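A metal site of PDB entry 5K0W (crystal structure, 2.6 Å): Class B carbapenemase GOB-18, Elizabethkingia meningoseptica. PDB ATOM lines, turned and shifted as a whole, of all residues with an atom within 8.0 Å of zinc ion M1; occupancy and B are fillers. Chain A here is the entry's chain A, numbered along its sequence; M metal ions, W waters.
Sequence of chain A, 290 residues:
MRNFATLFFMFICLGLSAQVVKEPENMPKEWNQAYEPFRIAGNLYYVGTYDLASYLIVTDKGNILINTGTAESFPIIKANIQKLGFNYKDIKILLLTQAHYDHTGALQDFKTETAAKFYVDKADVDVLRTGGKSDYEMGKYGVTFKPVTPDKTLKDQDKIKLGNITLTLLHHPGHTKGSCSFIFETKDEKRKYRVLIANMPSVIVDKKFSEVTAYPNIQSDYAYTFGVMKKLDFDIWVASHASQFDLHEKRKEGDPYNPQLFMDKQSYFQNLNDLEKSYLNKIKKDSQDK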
ATOM      1  N   TRP A  31       6.874 -13.018  -4.023  1.00  0.00           N
ATOM      2  CA  TRP A  31       5.422 -12.870  -3.984  1.00  0.00           C
ATOM      3  C   TRP A  31       4.673 -13.837  -4.878  1.00  0.00           C
ATOM      4  O   TRP A  31       3.601 -14.322  -4.496  1.00  0.00           O
ATOM      5  CB  TRP A  31       5.017 -11.423  -4.285  1.00  0.00           C
ATOM      6  CG  TRP A  31       5.216 -10.481  -3.135  1.00  0.00           C
ATOM      7  CD1 TRP A  31       6.002 -10.668  -2.027  1.00  0.00           C
ATOM      8  CD2 TRP A  31       4.639  -9.180  -3.006  1.00  0.00           C
ATOM      9  NE1 TRP A  31       5.952  -9.563  -1.220  1.00  0.00           N
ATOM     10  CE2 TRP A  31       5.135  -8.628  -1.801  1.00  0.00           C
ATOM     11  CE3 TRP A  31       3.787  -8.406  -3.811  1.00  0.00           C
ATOM     12  CZ2 TRP A  31       4.770  -7.348  -1.354  1.00  0.00           C
ATOM     13  CZ3 TRP A  31       3.439  -7.137  -3.378  1.00  0.00           C
ATOM     14  CH2 TRP A  31       3.903  -6.624  -2.153  1.00  0.00           C
ATOM     15  N   THR A  97      -7.030 -10.239   5.868  1.00  0.00           N
ATOM     16  CA  THR A  97      -6.341  -9.587   6.993  1.00  0.00           C
ATOM     17  C   THR A  97      -6.065  -8.105   6.681  1.00  0.00           C
ATOM     18  O   THR A  97      -5.821  -7.336   7.603  1.00  0.00           O
ATOM     19  CB  THR A  97      -5.083 -10.342   7.442  1.00  0.00           C
ATOM     20  OG1 THR A  97      -4.180 -10.460   6.354  1.00  0.00           O
ATOM     21  CG2 THR A  97      -5.400 -11.709   8.044  1.00  0.00           C
ATOM     22  N   GLN A  98      -6.083  -7.732   5.375  1.00  0.00           N
ATOM     23  CA  GLN A  98      -5.841  -6.386   4.874  1.00  0.00           C
ATOM     24  C   GLN A  98      -6.278  -6.282   3.397  1.00  0.00           C
ATOM     25  O   GLN A  98      -6.126  -7.246   2.643  1.00  0.00           O
ATOM     26  CB  GLN A  98      -4.346  -5.982   5.032  1.00  0.00           C
ATOM     27  CG  GLN A  98      -3.355  -6.977   4.436  1.00  0.00           C
ATOM     28  CD  GLN A  98      -1.976  -6.387   4.293  1.00  0.00           C
ATOM     29  OE1 GLN A  98      -1.709  -5.605   3.366  1.00  0.00           O
ATOM     30  NE2 GLN A  98      -1.052  -6.813   5.166  1.00  0.00           N
ATOM     31  N   ALA A  99      -6.823  -5.094   2.980  1.00  0.00           N
ATOM     32  CA  ALA A  99      -7.315  -4.862   1.612  1.00  0.00           C
ATOM     33  C   ALA A  99      -6.287  -4.261   0.660  1.00  0.00           C
ATOM     34  O   ALA A  99      -6.478  -3.166   0.116  1.00  0.00           O
ATOM     35  CB  ALA A  99      -8.593  -4.027   1.640  1.00  0.00           C
ATOM     36  N   HIS A 100      -5.187  -5.014   0.449  1.00  0.00           N
ATOM     37  CA  HIS A 100      -4.125  -4.694  -0.499  1.00  0.00           C
ATOM     38  C   HIS A 100      -4.058  -5.805  -1.536  1.00  0.00           C
ATOM     39  O   HIS A 100      -4.270  -6.968  -1.168  1.00  0.00           O
ATOM     40  CB  HIS A 100      -2.791  -4.525   0.216  1.00  0.00           C
ATOM     41  CG  HIS A 100      -2.618  -3.220   0.922  1.00  0.00           C
ATOM     42  ND1 HIS A 100      -1.701  -3.069   1.933  1.00  0.00           N
ATOM     43  CD2 HIS A 100      -3.255  -2.043   0.725  1.00  0.00           C
ATOM     44  CE1 HIS A 100      -1.812  -1.813   2.322  1.00  0.00           C
ATOM     45  NE2 HIS A 100      -2.713  -1.155   1.612  1.00  0.00           N
ATOM     46  N   TYR A 101      -3.787  -5.462  -2.815  1.00  0.00           N
ATOM     47  CA  TYR A 101      -3.698  -6.388  -3.972  1.00  0.00           C
ATOM     48  C   TYR A 101      -2.889  -7.682  -3.709  1.00  0.00           C
ATOM     49  O   TYR A 101      -3.207  -8.713  -4.298  1.00  0.00           O
ATOM     50  CB  TYR A 101      -3.211  -5.671  -5.254  1.00  0.00           C
ATOM     51  CG  TYR A 101      -1.720  -5.446  -5.306  1.00  0.00           C
ATOM     52  CD1 TYR A 101      -1.134  -4.387  -4.627  1.00  0.00           C
ATOM     53  CD2 TYR A 101      -0.890  -6.286  -6.047  1.00  0.00           C
ATOM     54  CE1 TYR A 101       0.245  -4.187  -4.653  1.00  0.00           C
ATOM     55  CE2 TYR A 101       0.497  -6.075  -6.094  1.00  0.00           C
ATOM     56  CZ  TYR A 101       1.057  -5.027  -5.380  1.00  0.00           C
ATOM     57  OH  TYR A 101       2.406  -4.810  -5.420  1.00  0.00           O
ATOM     58  N   ASP A 102      -1.858  -7.603  -2.851  1.00  0.00           N
ATOM     59  CA  ASP A 102      -1.015  -8.747  -2.521  1.00  0.00           C
ATOM     60  C   ASP A 102      -1.695  -9.752  -1.555  1.00  0.00           C
ATOM     61  O   ASP A 102      -1.089 -10.768  -1.206  1.00  0.00           O
ATOM     62  CB  ASP A 102       0.384  -8.306  -2.033  1.00  0.00           C
ATOM     63  CG  ASP A 102       0.393  -7.445  -0.800  1.00  0.00           C
ATOM     64  OD1 ASP A 102      -0.386  -6.459  -0.745  1.00  0.00           O
ATOM     65  OD2 ASP A 102       1.243  -7.699   0.102  1.00  0.00           O
ATOM     66  N   HIS A 103      -2.951  -9.506  -1.156  1.00  0.00           N
ATOM     67  CA  HIS A 103      -3.750 -10.425  -0.332  1.00  0.00           C
ATOM     68  C   HIS A 103      -5.174 -10.556  -0.903  1.00  0.00           C
ATOM     69  O   HIS A 103      -5.917 -11.454  -0.495  1.00  0.00           O
ATOM     70  CB  HIS A 103      -3.802  -9.981   1.148  1.00  0.00           C
ATOM     71  CG  HIS A 103      -2.459  -9.633   1.724  1.00  0.00           C
ATOM     72  ND1 HIS A 103      -1.634 -10.606   2.268  1.00  0.00           N
ATOM     73  CD2 HIS A 103      -1.823  -8.447   1.778  1.00  0.00           C
ATOM     74  CE1 HIS A 103      -0.538  -9.970   2.642  1.00  0.00           C
ATOM     75  NE2 HIS A 103      -0.617  -8.671   2.375  1.00  0.00           N
ATOM     76  N   ASP A 135      -8.157   3.430  -1.707  1.00  0.00           N
ATOM     77  CA  ASP A 135      -7.083   3.251  -0.710  1.00  0.00           C
ATOM     78  C   ASP A 135      -6.297   4.547  -0.492  1.00  0.00           C
ATOM     79  O   ASP A 135      -5.827   5.148  -1.460  1.00  0.00           O
ATOM     80  CB  ASP A 135      -6.143   2.094  -1.086  1.00  0.00           C
ATOM     81  CG  ASP A 135      -5.264   1.622   0.066  1.00  0.00           C
ATOM     82  OD1 ASP A 135      -4.281   2.333   0.389  1.00  0.00           O
ATOM     83  OD2 ASP A 135      -5.556   0.549   0.646  1.00  0.00           O
ATOM     84  N   TYR A 136      -6.163   4.974   0.789  1.00  0.00           N
ATOM     85  CA  TYR A 136      -5.440   6.172   1.229  1.00  0.00           C
ATOM     86  C   TYR A 136      -3.997   6.234   0.730  1.00  0.00           C
ATOM     87  O   TYR A 136      -3.393   7.315   0.691  1.00  0.00           O
ATOM     88  CB  TYR A 136      -5.514   6.307   2.759  1.00  0.00           C
ATOM     89  CG  TYR A 136      -4.610   5.378   3.521  1.00  0.00           C
ATOM     90  CD1 TYR A 136      -4.971   4.061   3.759  1.00  0.00           C
ATOM     91  CD2 TYR A 136      -3.390   5.825   4.031  1.00  0.00           C
ATOM     92  CE1 TYR A 136      -4.143   3.208   4.494  1.00  0.00           C
ATOM     93  CE2 TYR A 136      -2.540   4.973   4.721  1.00  0.00           C
ATOM     94  CZ  TYR A 136      -2.914   3.661   4.942  1.00  0.00           C
ATOM     95  OH  TYR A 136      -2.085   2.840   5.661  1.00  0.00           O
ATOM     96  N   MET A 138      -2.681   3.165  -1.644  1.00  0.00           N
ATOM     97  CA  MET A 138      -2.682   2.342  -2.863  1.00  0.00           C
ATOM     98  C   MET A 138      -3.566   2.856  -4.018  1.00  0.00           C
ATOM     99  O   MET A 138      -3.453   2.349  -5.138  1.00  0.00           O
ATOM    100  CB  MET A 138      -2.983   0.871  -2.525  1.00  0.00           C
ATOM    101  CG  MET A 138      -1.986   0.249  -1.559  1.00  0.00           C
ATOM    102  SD  MET A 138      -0.280   0.390  -2.134  1.00  0.00           S
ATOM    103  CE  MET A 138      -0.310  -0.782  -3.470  1.00  0.00           C
ATOM    104  N   HIS A 175      -2.579  -0.318   8.944  1.00  0.00           N
ATOM    105  CA  HIS A 175      -1.987  -0.754   7.699  1.00  0.00           C
ATOM    106  C   HIS A 175      -2.967  -0.489   6.545  1.00  0.00           C
ATOM    107  O   HIS A 175      -2.580  -0.035   5.467  1.00  0.00           O
ATOM    108  CB  HIS A 175      -1.542  -2.214   7.796  1.00  0.00           C
ATOM    109  CG  HIS A 175      -0.745  -2.670   6.615  1.00  0.00           C
ATOM    110  ND1 HIS A 175       0.634  -2.508   6.563  1.00  0.00           N
ATOM    111  CD2 HIS A 175      -1.172  -3.238   5.457  1.00  0.00           C
ATOM    112  CE1 HIS A 175       1.005  -3.009   5.389  1.00  0.00           C
ATOM    113  NE2 HIS A 175      -0.047  -3.460   4.685  1.00  0.00           N
ATOM    114  N   THR A 176      -4.242  -0.762   6.788  1.00  0.00           N
ATOM    115  CA  THR A 176      -5.418  -0.466   5.981  1.00  0.00           C
ATOM    116  C   THR A 176      -6.444  -0.021   7.046  1.00  0.00           C
ATOM    117  O   THR A 176      -6.252  -0.316   8.241  1.00  0.00           O
ATOM    118  CB  THR A 176      -5.906  -1.627   5.084  1.00  0.00           C
ATOM    119  OG1 THR A 176      -6.350  -2.702   5.886  1.00  0.00           O
ATOM    120  CG2 THR A 176      -4.871  -2.080   4.068  1.00  0.00           C
ATOM    121  N   SER A 179      -7.727  -3.349   8.461  1.00  0.00           N
ATOM    122  CA  SER A 179      -6.835  -4.501   8.628  1.00  0.00           C
ATOM    123  C   SER A 179      -7.248  -5.221   9.918  1.00  0.00           C
ATOM    124  O   SER A 179      -7.776  -4.592  10.830  1.00  0.00           O
ATOM    125  CB  SER A 179      -5.361  -4.107   8.634  1.00  0.00           C
ATOM    126  OG  SER A 179      -5.113  -2.811   9.151  1.00  0.00           O
ATOM    127  N   ASN A 199      -2.069  -9.462  11.477  1.00  0.00           N
ATOM    128  CA  ASN A 199      -1.736  -8.506  10.452  1.00  0.00           C
ATOM    129  C   ASN A 199      -0.877  -7.466  11.173  1.00  0.00           C
ATOM    130  O   ASN A 199      -1.403  -6.598  11.875  1.00  0.00           O
ATOM    131  CB  ASN A 199      -2.958  -7.891   9.761  1.00  0.00           C
ATOM    132  CG  ASN A 199      -2.553  -7.145   8.518  1.00  0.00           C
ATOM    133  OD1 ASN A 199      -2.273  -7.738   7.469  1.00  0.00           O
ATOM    134  ND2 ASN A 199      -2.340  -5.859   8.650  1.00  0.00           N
ATOM    135  N   MET A 200       0.449  -7.637  11.081  1.00  0.00           N
ATOM    136  CA  MET A 200       1.458  -6.804  11.715  1.00  0.00           C
ATOM    137  C   MET A 200       1.293  -5.312  11.399  1.00  0.00           C
ATOM    138  O   MET A 200       1.125  -4.952  10.230  1.00  0.00           O
ATOM    139  CB  MET A 200       2.896  -7.307  11.431  1.00  0.00           C
ATOM    140  CG  MET A 200       3.155  -8.749  11.881  1.00  0.00           C
ATOM    141  SD  MET A 200       2.678  -9.122  13.602  1.00  0.00           S
ATOM    142  CE  MET A 200       4.061  -8.336  14.554  1.00  0.00           C
ATOM    143  N   SER A 202       2.527  -2.377  10.437  1.00  0.00           N
ATOM    144  CA  SER A 202       3.576  -1.590   9.775  1.00  0.00           C
ATOM    145  C   SER A 202       3.002  -0.300   9.142  1.00  0.00           C
ATOM    146  O   SER A 202       1.806  -0.212   8.902  1.00  0.00           O
ATOM    147  CB  SER A 202       4.314  -2.440   8.731  1.00  0.00           C
ATOM    148  OG  SER A 202       3.421  -3.237   7.980  1.00  0.00           O
ATOM    149  N   ILE A 204       3.014   2.244   5.925  1.00  0.00           N
ATOM    150  CA  ILE A 204       3.256   2.328   4.469  1.00  0.00           C
ATOM    151  C   ILE A 204       3.405   3.758   3.905  1.00  0.00           C
ATOM    152  O   ILE A 204       3.876   3.930   2.771  1.00  0.00           O
ATOM    153  CB  ILE A 204       2.259   1.463   3.654  1.00  0.00           C
ATOM    154  CG1 ILE A 204       0.808   2.025   3.723  1.00  0.00           C
ATOM    155  CG2 ILE A 204       2.340   0.004   4.153  1.00  0.00           C
ATOM    156  CD1 ILE A 204      -0.198   1.354   2.836  1.00  0.00           C
ATOM    157  N   SER A 240       0.498 -12.103   7.676  1.00  0.00           N
ATOM    158  CA  SER A 240       0.172 -11.872   6.259  1.00  0.00           C
ATOM    159  C   SER A 240       1.325 -12.207   5.290  1.00  0.00           C
ATOM    160  O   SER A 240       1.100 -12.583   4.136  1.00  0.00           O
ATOM    161  CB  SER A 240      -0.257 -10.421   6.045  1.00  0.00           C
ATOM    162  OG  SER A 240      -1.487 -10.106   6.685  1.00  0.00           O
ATOM    163  N   HIS A 241       2.560 -12.033   5.757  1.00  0.00           N
ATOM    164  CA  HIS A 241       3.796 -12.305   5.009  1.00  0.00           C
ATOM    165  C   HIS A 241       4.662 -13.327   5.744  1.00  0.00           C
ATOM    166  O   HIS A 241       4.808 -13.253   6.970  1.00  0.00           O
ATOM    167  CB  HIS A 241       4.557 -11.014   4.790  1.00  0.00           C
ATOM    168  CG  HIS A 241       3.930 -10.110   3.781  1.00  0.00           C
ATOM    169  ND1 HIS A 241       4.393 -10.048   2.468  1.00  0.00           N
ATOM    170  CD2 HIS A 241       2.864  -9.290   3.903  1.00  0.00           C
ATOM    171  CE1 HIS A 241       3.611  -9.176   1.851  1.00  0.00           C
ATOM    172  NE2 HIS A 241       2.670  -8.713   2.658  1.00  0.00           N
ATOM    173  N   GLN A 244       7.586 -12.257   8.130  1.00  0.00           N
ATOM    174  CA  GLN A 244       7.175 -11.681   9.415  1.00  0.00           C
ATOM    175  C   GLN A 244       7.212 -12.671  10.565  1.00  0.00           C
ATOM    176  O   GLN A 244       7.536 -12.286  11.694  1.00  0.00           O
ATOM    177  CB  GLN A 244       5.807 -11.020   9.310  1.00  0.00           C
ATOM    178  CG  GLN A 244       5.837  -9.778   8.431  1.00  0.00           C
ATOM    179  CD  GLN A 244       4.474  -9.237   8.123  1.00  0.00           C
ATOM    180  OE1 GLN A 244       3.519  -9.980   7.862  1.00  0.00           O
ATOM    181  NE2 GLN A 244       4.342  -7.939   8.111  1.00  0.00           N
HETATM  182 ZN    ZN M   1      -0.277  -4.270   2.811  1.00  0.00          ZN
HETATM  183 ZN    ZN M   2       1.086  -7.453   2.186  1.00  0.00          ZN
HETATM  184  O   HOH W   1       1.312  -5.581   3.028  1.00  0.00           O
HETATM  185  O   HOH W   2       1.310  -3.002   1.931  1.00  0.00           O
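A ring nitrogen (NE2) of His 100 sits at hydrogen-bond distance from the side-chain carboxylate (OD2) of Asp 135, 3.5 Å away. The side-chain amide oxygen (OD1) of Asn 199 is in hydrogen-bond range of the side-chain amide nitrogen (NE2) of Gln 98 (2.8 Å). The side-chain hydroxyl (OH) of Tyr 136 lies within hydrogen-bond range of the backbone carbonyl oxygen (O) of His 175. The side-chain amide nitrogen (NE2) of Gln 98 sits close to a ring nitrogen (NE2) of His 103 (3.4 Å). ND1 of His 175 sits at hydrogen-bond distance from OG of Ser 202, at 3.2 Å.
The nearest printed residue that does not touch zinc ion M1 is Asp 102 (4.2 Å).
Zinc ion M1 is bound by OE1 of Gln 98, NE2 of His 175, ND1 of His 100, water W1 and water W2.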
